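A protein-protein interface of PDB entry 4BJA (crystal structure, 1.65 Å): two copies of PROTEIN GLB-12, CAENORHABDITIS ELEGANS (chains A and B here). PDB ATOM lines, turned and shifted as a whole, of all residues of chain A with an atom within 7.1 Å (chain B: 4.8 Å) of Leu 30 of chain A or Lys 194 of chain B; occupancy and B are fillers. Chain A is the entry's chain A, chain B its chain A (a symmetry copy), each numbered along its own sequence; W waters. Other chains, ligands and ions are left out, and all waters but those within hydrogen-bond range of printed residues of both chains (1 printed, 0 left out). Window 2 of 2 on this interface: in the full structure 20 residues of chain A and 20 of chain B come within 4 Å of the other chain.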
ATOM      1  N   SER A  24      35.900 -25.996   3.160  1.00  0.00           N
ATOM      2  CA  SER A  24      34.481 -25.785   3.407  1.00  0.00           C
ATOM      3  C   SER A  24      33.785 -25.021   2.268  1.00  0.00           C
ATOM      4  O   SER A  24      32.567 -24.960   2.227  1.00  0.00           O
ATOM      5  CB  SER A  24      34.269 -25.037   4.749  1.00  0.00           C
ATOM      6  OG  SER A  24      34.980 -23.827   4.726  1.00  0.00           O
ATOM      7  N   GLU A  25      34.547 -24.483   1.319  1.00  0.00           N
ATOM      8  CA  GLU A  25      33.946 -23.673   0.258  1.00  0.00           C
ATOM      9  C   GLU A  25      33.557 -24.528  -0.940  1.00  0.00           C
ATOM     10  O   GLU A  25      33.155 -24.014  -1.968  1.00  0.00           O
ATOM     11  CB  GLU A  25      34.899 -22.557  -0.180  1.00  0.00           C
ATOM     12  CG  GLU A  25      35.204 -21.590   0.958  1.00  0.00           C
ATOM     13  CD  GLU A  25      36.474 -21.936   1.744  1.00  0.00           C
ATOM     14  OE1 GLU A  25      36.948 -23.048   1.688  1.00  0.00           O
ATOM     15  OE2 GLU A  25      36.997 -21.063   2.436  1.00  0.00           O
ATOM     16  N   ASN A  26      33.640 -25.837  -0.771  1.00  0.00           N
ATOM     17  CA  ASN A  26      33.349 -26.797  -1.886  1.00  0.00           C
ATOM     18  C   ASN A  26      31.925 -26.550  -2.424  1.00  0.00           C
ATOM     19  O   ASN A  26      30.980 -26.700  -1.688  1.00  0.00           O
ATOM     20  CB  ASN A  26      33.402 -28.190  -1.227  1.00  0.00           C
ATOM     21  CG  ASN A  26      33.199 -29.325  -2.169  1.00  0.00           C
ATOM     22  OD1 ASN A  26      32.529 -29.216  -3.215  1.00  0.00           O
ATOM     23  ND2 ASN A  26      33.732 -30.474  -1.781  1.00  0.00           N
ATOM     24  N   PRO A  27      31.764 -26.193  -3.711  1.00  0.00           N
ATOM     25  CA  PRO A  27      30.423 -25.792  -4.169  1.00  0.00           C
ATOM     26  C   PRO A  27      29.477 -26.969  -4.241  1.00  0.00           C
ATOM     27  O   PRO A  27      28.286 -26.773  -4.236  1.00  0.00           O
ATOM     28  CB  PRO A  27      30.672 -25.190  -5.559  1.00  0.00           C
ATOM     29  CG  PRO A  27      31.945 -25.885  -6.028  1.00  0.00           C
ATOM     30  CD  PRO A  27      32.788 -26.001  -4.743  1.00  0.00           C
ATOM     31  N   PHE A  28      30.008 -28.192  -4.284  1.00  0.00           N
ATOM     32  CA  PHE A  28      29.141 -29.349  -4.278  1.00  0.00           C
ATOM     33  C   PHE A  28      28.536 -29.553  -2.905  1.00  0.00           C
ATOM     34  O   PHE A  28      27.512 -30.215  -2.757  1.00  0.00           O
ATOM     35  CB  PHE A  28      29.892 -30.617  -4.745  1.00  0.00           C
ATOM     36  CG  PHE A  28      30.274 -30.570  -6.166  1.00  0.00           C
ATOM     37  CD1 PHE A  28      29.306 -30.835  -7.131  1.00  0.00           C
ATOM     38  CD2 PHE A  28      31.560 -30.202  -6.556  1.00  0.00           C
ATOM     39  CE1 PHE A  28      29.642 -30.744  -8.489  1.00  0.00           C
ATOM     40  CE2 PHE A  28      31.911 -30.106  -7.904  1.00  0.00           C
ATOM     41  CZ  PHE A  28      30.923 -30.388  -8.874  1.00  0.00           C
ATOM     42  N   ASP A  29      29.184 -29.024  -1.875  1.00  0.00           N
ATOM     43  CA  ASP A  29      28.543 -29.064  -0.577  1.00  0.00           C
ATOM     44  C   ASP A  29      27.612 -27.891  -0.391  1.00  0.00           C
ATOM     45  O   ASP A  29      26.662 -28.006   0.366  1.00  0.00           O
ATOM     46  CB  ASP A  29      29.604 -29.136   0.537  1.00  0.00           C
ATOM     47  CG  ASP A  29      28.981 -29.412   1.914  1.00  0.00           C
ATOM     48  OD1 ASP A  29      27.904 -30.049   2.009  1.00  0.00           O
ATOM     49  OD2 ASP A  29      29.567 -28.947   2.915  1.00  0.00           O
ATOM     50  N   LEU A  30      27.875 -26.764  -1.048  1.00  0.00           N
ATOM     51  CA  LEU A  30      27.032 -25.573  -0.894  1.00  0.00           C
ATOM     52  C   LEU A  30      25.758 -25.568  -1.735  1.00  0.00           C
ATOM     53  O   LEU A  30      24.687 -25.141  -1.274  1.00  0.00           O
ATOM     54  CB  LEU A  30      27.862 -24.321  -1.198  1.00  0.00           C
ATOM     55  CG  LEU A  30      29.130 -24.188  -0.346  1.00  0.00           C
ATOM     56  CD1 LEU A  30      29.832 -22.900  -0.747  1.00  0.00           C
ATOM     57  CD2 LEU A  30      28.836 -24.218   1.164  1.00  0.00           C
ATOM     58  N   ALA A  31      25.865 -26.090  -2.952  1.00  0.00           N
ATOM     59  CA  ALA A  31      24.728 -26.111  -3.893  1.00  0.00           C
ATOM     60  C   ALA A  31      23.825 -27.303  -3.682  1.00  0.00           C
ATOM     61  O   ALA A  31      22.655 -27.290  -4.133  1.00  0.00           O
ATOM     62  CB  ALA A  31      25.261 -26.081  -5.339  1.00  0.00           C
ATOM     63  N   LEU A  32      24.351 -28.347  -3.045  1.00  0.00           N
ATOM     64  CA  LEU A  32      23.629 -29.606  -2.912  1.00  0.00           C
ATOM     65  C   LEU A  32      23.686 -29.904  -1.441  1.00  0.00           C
ATOM     66  O   LEU A  32      24.676 -29.567  -0.803  1.00  0.00           O
ATOM     67  CB  LEU A  32      24.361 -30.690  -3.702  1.00  0.00           C
ATOM     68  CG  LEU A  32      24.445 -30.385  -5.207  1.00  0.00           C
ATOM     69  CD1 LEU A  32      25.530 -31.311  -5.816  1.00  0.00           C
ATOM     70  CD2 LEU A  32      23.026 -30.524  -5.877  1.00  0.00           C
ATOM     71  N   ASN A  33      22.593 -30.375  -0.892  1.00  0.00           N
ATOM     72  CA  ASN A  33      22.611 -30.871   0.459  1.00  0.00           C
ATOM     73  C   ASN A  33      22.620 -32.399   0.412  1.00  0.00           C
ATOM     74  O   ASN A  33      22.721 -33.008  -0.674  1.00  0.00           O
ATOM     75  CB  ASN A  33      21.438 -30.242   1.246  1.00  0.00           C
ATOM     76  CG  ASN A  33      20.058 -30.675   0.748  1.00  0.00           C
ATOM     77  OD1 ASN A  33      19.883 -31.715   0.097  1.00  0.00           O
ATOM     78  ND2 ASN A  33      19.050 -29.884   1.098  1.00  0.00           N
ATOM     79  N   ASP A  36      19.751 -33.904  -1.607  1.00  0.00           N
ATOM     80  CA  ASP A  36      19.997 -33.640  -3.042  1.00  0.00           C
ATOM     81  C   ASP A  36      20.983 -34.667  -3.591  1.00  0.00           C
ATOM     82  O   ASP A  36      20.809 -35.193  -4.701  1.00  0.00           O
ATOM     83  CB  ASP A  36      20.617 -32.250  -3.274  1.00  0.00           C
ATOM     84  CG  ASP A  36      19.677 -31.105  -2.921  1.00  0.00           C
ATOM     85  OD1 ASP A  36      18.452 -31.332  -2.800  1.00  0.00           O
ATOM     86  OD2 ASP A  36      20.190 -29.960  -2.775  1.00  0.00           O
ATOM     87  N   LEU A 113      32.917 -35.687  -0.398  1.00  0.00           N
ATOM     88  CA  LEU A 113      32.714 -34.421  -1.092  1.00  0.00           C
ATOM     89  C   LEU A 113      34.073 -33.881  -1.583  1.00  0.00           C
ATOM     90  O   LEU A 113      34.154 -33.252  -2.642  1.00  0.00           O
ATOM     91  CB  LEU A 113      31.930 -33.440  -0.194  1.00  0.00           C
ATOM     92  CG  LEU A 113      30.619 -34.015   0.391  1.00  0.00           C
ATOM     93  CD1 LEU A 113      29.709 -32.922   0.946  1.00  0.00           C
ATOM     94  CD2 LEU A 113      29.813 -34.877  -0.645  1.00  0.00           C
ATOM     95  N   LYS A 194      21.327 -27.904 -10.714  1.00  0.00           N
ATOM     96  CA  LYS A 194      22.360 -27.355  -9.806  1.00  0.00           C
ATOM     97  C   LYS A 194      23.657 -28.130  -9.909  1.00  0.00           C
ATOM     98  O   LYS A 194      24.735 -27.537  -9.983  1.00  0.00           O
ATOM     99  CB  LYS A 194      21.878 -27.342  -8.367  1.00  0.00           C
ATOM    100  CG  LYS A 194      20.790 -26.295  -8.168  1.00  0.00           C
ATOM    101  CD  LYS A 194      20.432 -26.183  -6.654  1.00  0.00           C
ATOM    102  CE  LYS A 194      20.073 -27.521  -5.990  1.00  0.00           C
ATOM    103  NZ  LYS A 194      19.861 -27.393  -4.474  1.00  0.00           N
ATOM    104  N   ALA B  31      23.726 -21.888  -4.885  1.00  0.00           N
ATOM    105  CA  ALA B  31      23.849 -22.150  -3.438  1.00  0.00           C
ATOM    106  C   ALA B  31      22.730 -21.523  -2.639  1.00  0.00           C
ATOM    107  O   ALA B  31      22.483 -21.933  -1.481  1.00  0.00           O
ATOM    108  CB  ALA B  31      25.219 -21.649  -2.942  1.00  0.00           C
ATOM    109  N   LEU B  32      22.079 -20.515  -3.213  1.00  0.00           N
ATOM    110  CA  LEU B  32      21.082 -19.736  -2.489  1.00  0.00           C
ATOM    111  C   LEU B  32      19.879 -19.758  -3.388  1.00  0.00           C
ATOM    112  O   LEU B  32      20.042 -19.772  -4.602  1.00  0.00           O
ATOM    113  CB  LEU B  32      21.591 -18.305  -2.319  1.00  0.00           C
ATOM    114  CG  LEU B  32      22.894 -18.222  -1.505  1.00  0.00           C
ATOM    115  CD1 LEU B  32      23.512 -16.821  -1.747  1.00  0.00           C
ATOM    116  CD2 LEU B  32      22.620 -18.557   0.009  1.00  0.00           C
ATOM    117  N   ASP B  36      16.325 -17.850   0.517  1.00  0.00           N
ATOM    118  CA  ASP B  36      17.641 -17.678   1.172  1.00  0.00           C
ATOM    119  C   ASP B  36      18.121 -16.242   0.990  1.00  0.00           C
ATOM    120  O   ASP B  36      18.646 -15.617   1.924  1.00  0.00           O
ATOM    121  CB  ASP B  36      18.714 -18.595   0.559  1.00  0.00           C
ATOM    122  CG  ASP B  36      18.454 -20.075   0.804  1.00  0.00           C
ATOM    123  OD1 ASP B  36      17.647 -20.416   1.699  1.00  0.00           O
ATOM    124  OD2 ASP B  36      19.087 -20.900   0.086  1.00  0.00           O
ATOM    125  N   ASP B 190      22.843 -21.450   8.518  1.00  0.00           N
ATOM    126  CA  ASP B 190      23.179 -22.224   7.338  1.00  0.00           C
ATOM    127  C   ASP B 190      23.231 -21.311   6.092  1.00  0.00           C
ATOM    128  O   ASP B 190      24.148 -21.431   5.282  1.00  0.00           O
ATOM    129  CB  ASP B 190      22.193 -23.402   7.151  1.00  0.00           C
ATOM    130  CG  ASP B 190      22.185 -24.398   8.341  1.00  0.00           C
ATOM    131  OD1 ASP B 190      22.985 -24.301   9.293  1.00  0.00           O
ATOM    132  OD2 ASP B 190      21.312 -25.298   8.333  1.00  0.00           O
ATOM    133  N   VAL B 191      22.281 -20.385   5.963  1.00  0.00           N
ATOM    134  CA  VAL B 191      22.257 -19.503   4.807  1.00  0.00           C
ATOM    135  C   VAL B 191      23.479 -18.583   4.780  1.00  0.00           C
ATOM    136  O   VAL B 191      24.110 -18.408   3.720  1.00  0.00           O
ATOM    137  CB  VAL B 191      20.941 -18.684   4.719  1.00  0.00           C
ATOM    138  CG1 VAL B 191      21.050 -17.666   3.640  1.00  0.00           C
ATOM    139  CG2 VAL B 191      19.758 -19.622   4.432  1.00  0.00           C
ATOM    140  N   TRP B 192      23.817 -18.000   5.938  1.00  0.00           N
ATOM    141  CA  TRP B 192      24.952 -17.101   5.981  1.00  0.00           C
ATOM    142  C   TRP B 192      26.235 -17.874   5.735  1.00  0.00           C
ATOM    143  O   TRP B 192      27.166 -17.369   5.102  1.00  0.00           O
ATOM    144  CB  TRP B 192      24.974 -16.294   7.324  1.00  0.00           C
ATOM    145  CG  TRP B 192      24.183 -15.051   7.173  1.00  0.00           C
ATOM    146  CD1 TRP B 192      22.856 -14.880   7.461  1.00  0.00           C
ATOM    147  CD2 TRP B 192      24.639 -13.815   6.625  1.00  0.00           C
ATOM    148  NE1 TRP B 192      22.462 -13.600   7.144  1.00  0.00           N
ATOM    149  CE2 TRP B 192      23.544 -12.919   6.638  1.00  0.00           C
ATOM    150  CE3 TRP B 192      25.878 -13.362   6.158  1.00  0.00           C
ATOM    151  CZ2 TRP B 192      23.657 -11.594   6.181  1.00  0.00           C
ATOM    152  CZ3 TRP B 192      25.989 -12.049   5.716  1.00  0.00           C
ATOM    153  CH2 TRP B 192      24.878 -11.185   5.713  1.00  0.00           C
ATOM    154  N   LYS B 193      26.320 -19.104   6.235  1.00  0.00           N
ATOM    155  CA  LYS B 193      27.514 -19.913   5.906  1.00  0.00           C
ATOM    156  C   LYS B 193      27.620 -20.192   4.404  1.00  0.00           C
ATOM    157  O   LYS B 193      28.702 -20.086   3.853  1.00  0.00           O
ATOM    158  CB  LYS B 193      27.601 -21.197   6.723  1.00  0.00           C
ATOM    159  CG  LYS B 193      27.951 -20.897   8.194  1.00  0.00           C
ATOM    160  CD  LYS B 193      28.057 -22.192   9.000  1.00  0.00           C
ATOM    161  CE  LYS B 193      28.391 -21.912  10.463  1.00  0.00           C
ATOM    162  NZ  LYS B 193      28.270 -23.185  11.321  1.00  0.00           N
ATOM    163  N   LYS B 194      26.501 -20.567   3.757  1.00  0.00           N
ATOM    164  CA  LYS B 194      26.573 -20.807   2.297  1.00  0.00           C
ATOM    165  C   LYS B 194      26.981 -19.555   1.550  1.00  0.00           C
ATOM    166  O   LYS B 194      27.833 -19.609   0.660  1.00  0.00           O
ATOM    167  CB  LYS B 194      25.252 -21.324   1.760  1.00  0.00           C
ATOM    168  CG  LYS B 194      24.991 -22.748   2.233  1.00  0.00           C
ATOM    169  CD  LYS B 194      23.718 -23.316   1.533  1.00  0.00           C
ATOM    170  CE  LYS B 194      22.473 -22.425   1.670  1.00  0.00           C
ATOM    171  NZ  LYS B 194      21.279 -22.946   0.856  1.00  0.00           N
ATOM    172  N   PHE B 195      26.388 -18.422   1.945  1.00  0.00           N
ATOM    173  CA  PHE B 195      26.671 -17.172   1.329  1.00  0.00           C
ATOM    174  C   PHE B 195      28.150 -16.796   1.503  1.00  0.00           C
ATOM    175  O   PHE B 195      28.872 -16.494   0.530  1.00  0.00           O
ATOM    176  CB  PHE B 195      25.726 -16.074   1.918  1.00  0.00           C
ATOM    177  CG  PHE B 195      26.112 -14.667   1.546  1.00  0.00           C
ATOM    178  CD1 PHE B 195      26.231 -14.280   0.200  1.00  0.00           C
ATOM    179  CD2 PHE B 195      26.379 -13.718   2.548  1.00  0.00           C
ATOM    180  CE1 PHE B 195      26.609 -12.979  -0.169  1.00  0.00           C
ATOM    181  CE2 PHE B 195      26.776 -12.415   2.182  1.00  0.00           C
ATOM    182  CZ  PHE B 195      26.876 -12.037   0.822  1.00  0.00           C
ATOM    183  N   LEU B 196      28.609 -16.778   2.748  1.00  0.00           N
ATOM    184  CA  LEU B 196      29.966 -16.291   3.015  1.00  0.00           C
ATOM    185  C   LEU B 196      31.024 -17.241   2.418  1.00  0.00           C
ATOM    186  O   LEU B 196      32.085 -16.786   1.942  1.00  0.00           O
ATOM    187  CB  LEU B 196      30.140 -16.080   4.512  1.00  0.00           C
ATOM    188  CG  LEU B 196      29.364 -14.872   5.052  1.00  0.00           C
ATOM    189  CD1 LEU B 196      29.545 -14.841   6.539  1.00  0.00           C
ATOM    190  CD2 LEU B 196      29.860 -13.576   4.469  1.00  0.00           C
ATOM    191  N   ASN B 197      30.753 -18.553   2.432  1.00  0.00           N
ATOM    192  CA  ASN B 197      31.642 -19.499   1.759  1.00  0.00           C
ATOM    193  C   ASN B 197      31.707 -19.304   0.246  1.00  0.00           C
ATOM    194  O   ASN B 197      32.756 -19.471  -0.363  1.00  0.00           O
ATOM    195  CB  ASN B 197      31.281 -20.944   2.137  1.00  0.00           C
ATOM    196  CG  ASN B 197      31.798 -21.267   3.553  1.00  0.00           C
ATOM    197  OD1 ASN B 197      32.952 -20.972   3.849  1.00  0.00           O
ATOM    198  ND2 ASN B 197      30.996 -21.859   4.387  1.00  0.00           N
ATOM    199  N   THR B 198      30.587 -18.912  -0.335  1.00  0.00           N
ATOM    200  CA  THR B 198      30.577 -18.613  -1.770  1.00  0.00           C
ATOM    201  C   THR B 198      31.353 -17.312  -2.041  1.00  0.00           C
ATOM    202  O   THR B 198      32.043 -17.218  -3.053  1.00  0.00           O
ATOM    203  CB  THR B 198      29.128 -18.525  -2.316  1.00  0.00           C
ATOM    204  OG1 THR B 198      28.478 -19.779  -2.031  1.00  0.00           O
ATOM    205  CG2 THR B 198      29.121 -18.297  -3.812  1.00  0.00           C
HETATM  206  O   HOH W   1      34.801 -21.435   5.748  1.00  0.00           O
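O of Ala 31 of chain B sits at hydrogen-bond distance from NZ of Lys 194 of chain B (2.8 Å). OD2 of Asp 36 of chain B lies within salt-bridge range of NZ of Lys 194 of chain B, at 3.1 Å. ND2 of Asn 197 of chain B is in hydrogen-bond range of O of Lys 193 of chain B, 2.9 Å away. The backbone carbonyl oxygen of Lys 194 of chain B is in hydrogen-bond range of the side-chain hydroxyl of Thr 198 of chain B.
Among the printed residues, merely in contact across the chains: Leu 30 of chain A with Lys 194 of chain B, Glu 25 of chain A with Asn 197 of chain B, Ser 24 of chain A with Asn 197 of chain B, Leu 30 of chain A with Thr 198 of chain B, Leu 30 of chain A with Asn 197 of chain B and Leu 30 of chain A with Ala 31 of chain B.
Leu 30 of chain A touches just these residues of chain B: Ala 31 (3.8 Å), Lys 194 (3.5 Å), Asn 197 (3.8 Å) and Thr 198 (3.6 Å). Of chain A, only Leu 30 (3.5 Å) comes within 4 Å of Lys 194 of chain B. Printed residues of chain A within 4 Å of Ala 31 of chain B: Leu 30. Printed residues of chain A within 4 Å of Asn 197 of chain B: Ser 24 (3.6 Å), Glu 25 (3.5 Å) and Leu 30 (3.8 Å). Of the printed residues of chain B, Glu 25 of chain A touches Asn 197 (3.5 Å). Trp 192 of chain B touches none of the printed residues of chain A. The nearest printed residue of chain B that does not touch Leu 30 of chain A is Lys 193 of chain B (4.9 Å). The nearest residue of chain A that does not touch Lys 194 of chain B is Asp 29 of chain A (5.7 Å). The nearest printed residue of chain B that does not touch Ser 24 of chain A is Lys 193 of chain B (6.4 Å).
Hydrophobic or aromatic side chains of chain B within 4 Å of the printed part of chain A: Ala 31. Printed residues of chain A that touch a printed residue of chain B: Ser 24, Glu 25 and Leu 30. Hydrophobic or aromatic side chains of chain A within 4 Å of the printed part of chain B: Leu 30. Among the printed residues, 6 pairs touch across the chains.
Positions printed for both chains: 31, 32, 36 and 194.
Water W1 lies within hydrogen-bond range of OG of Ser 24 of chain A (2.6 Å) and OD1 of Asn 197 of chain B (2.7 Å).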
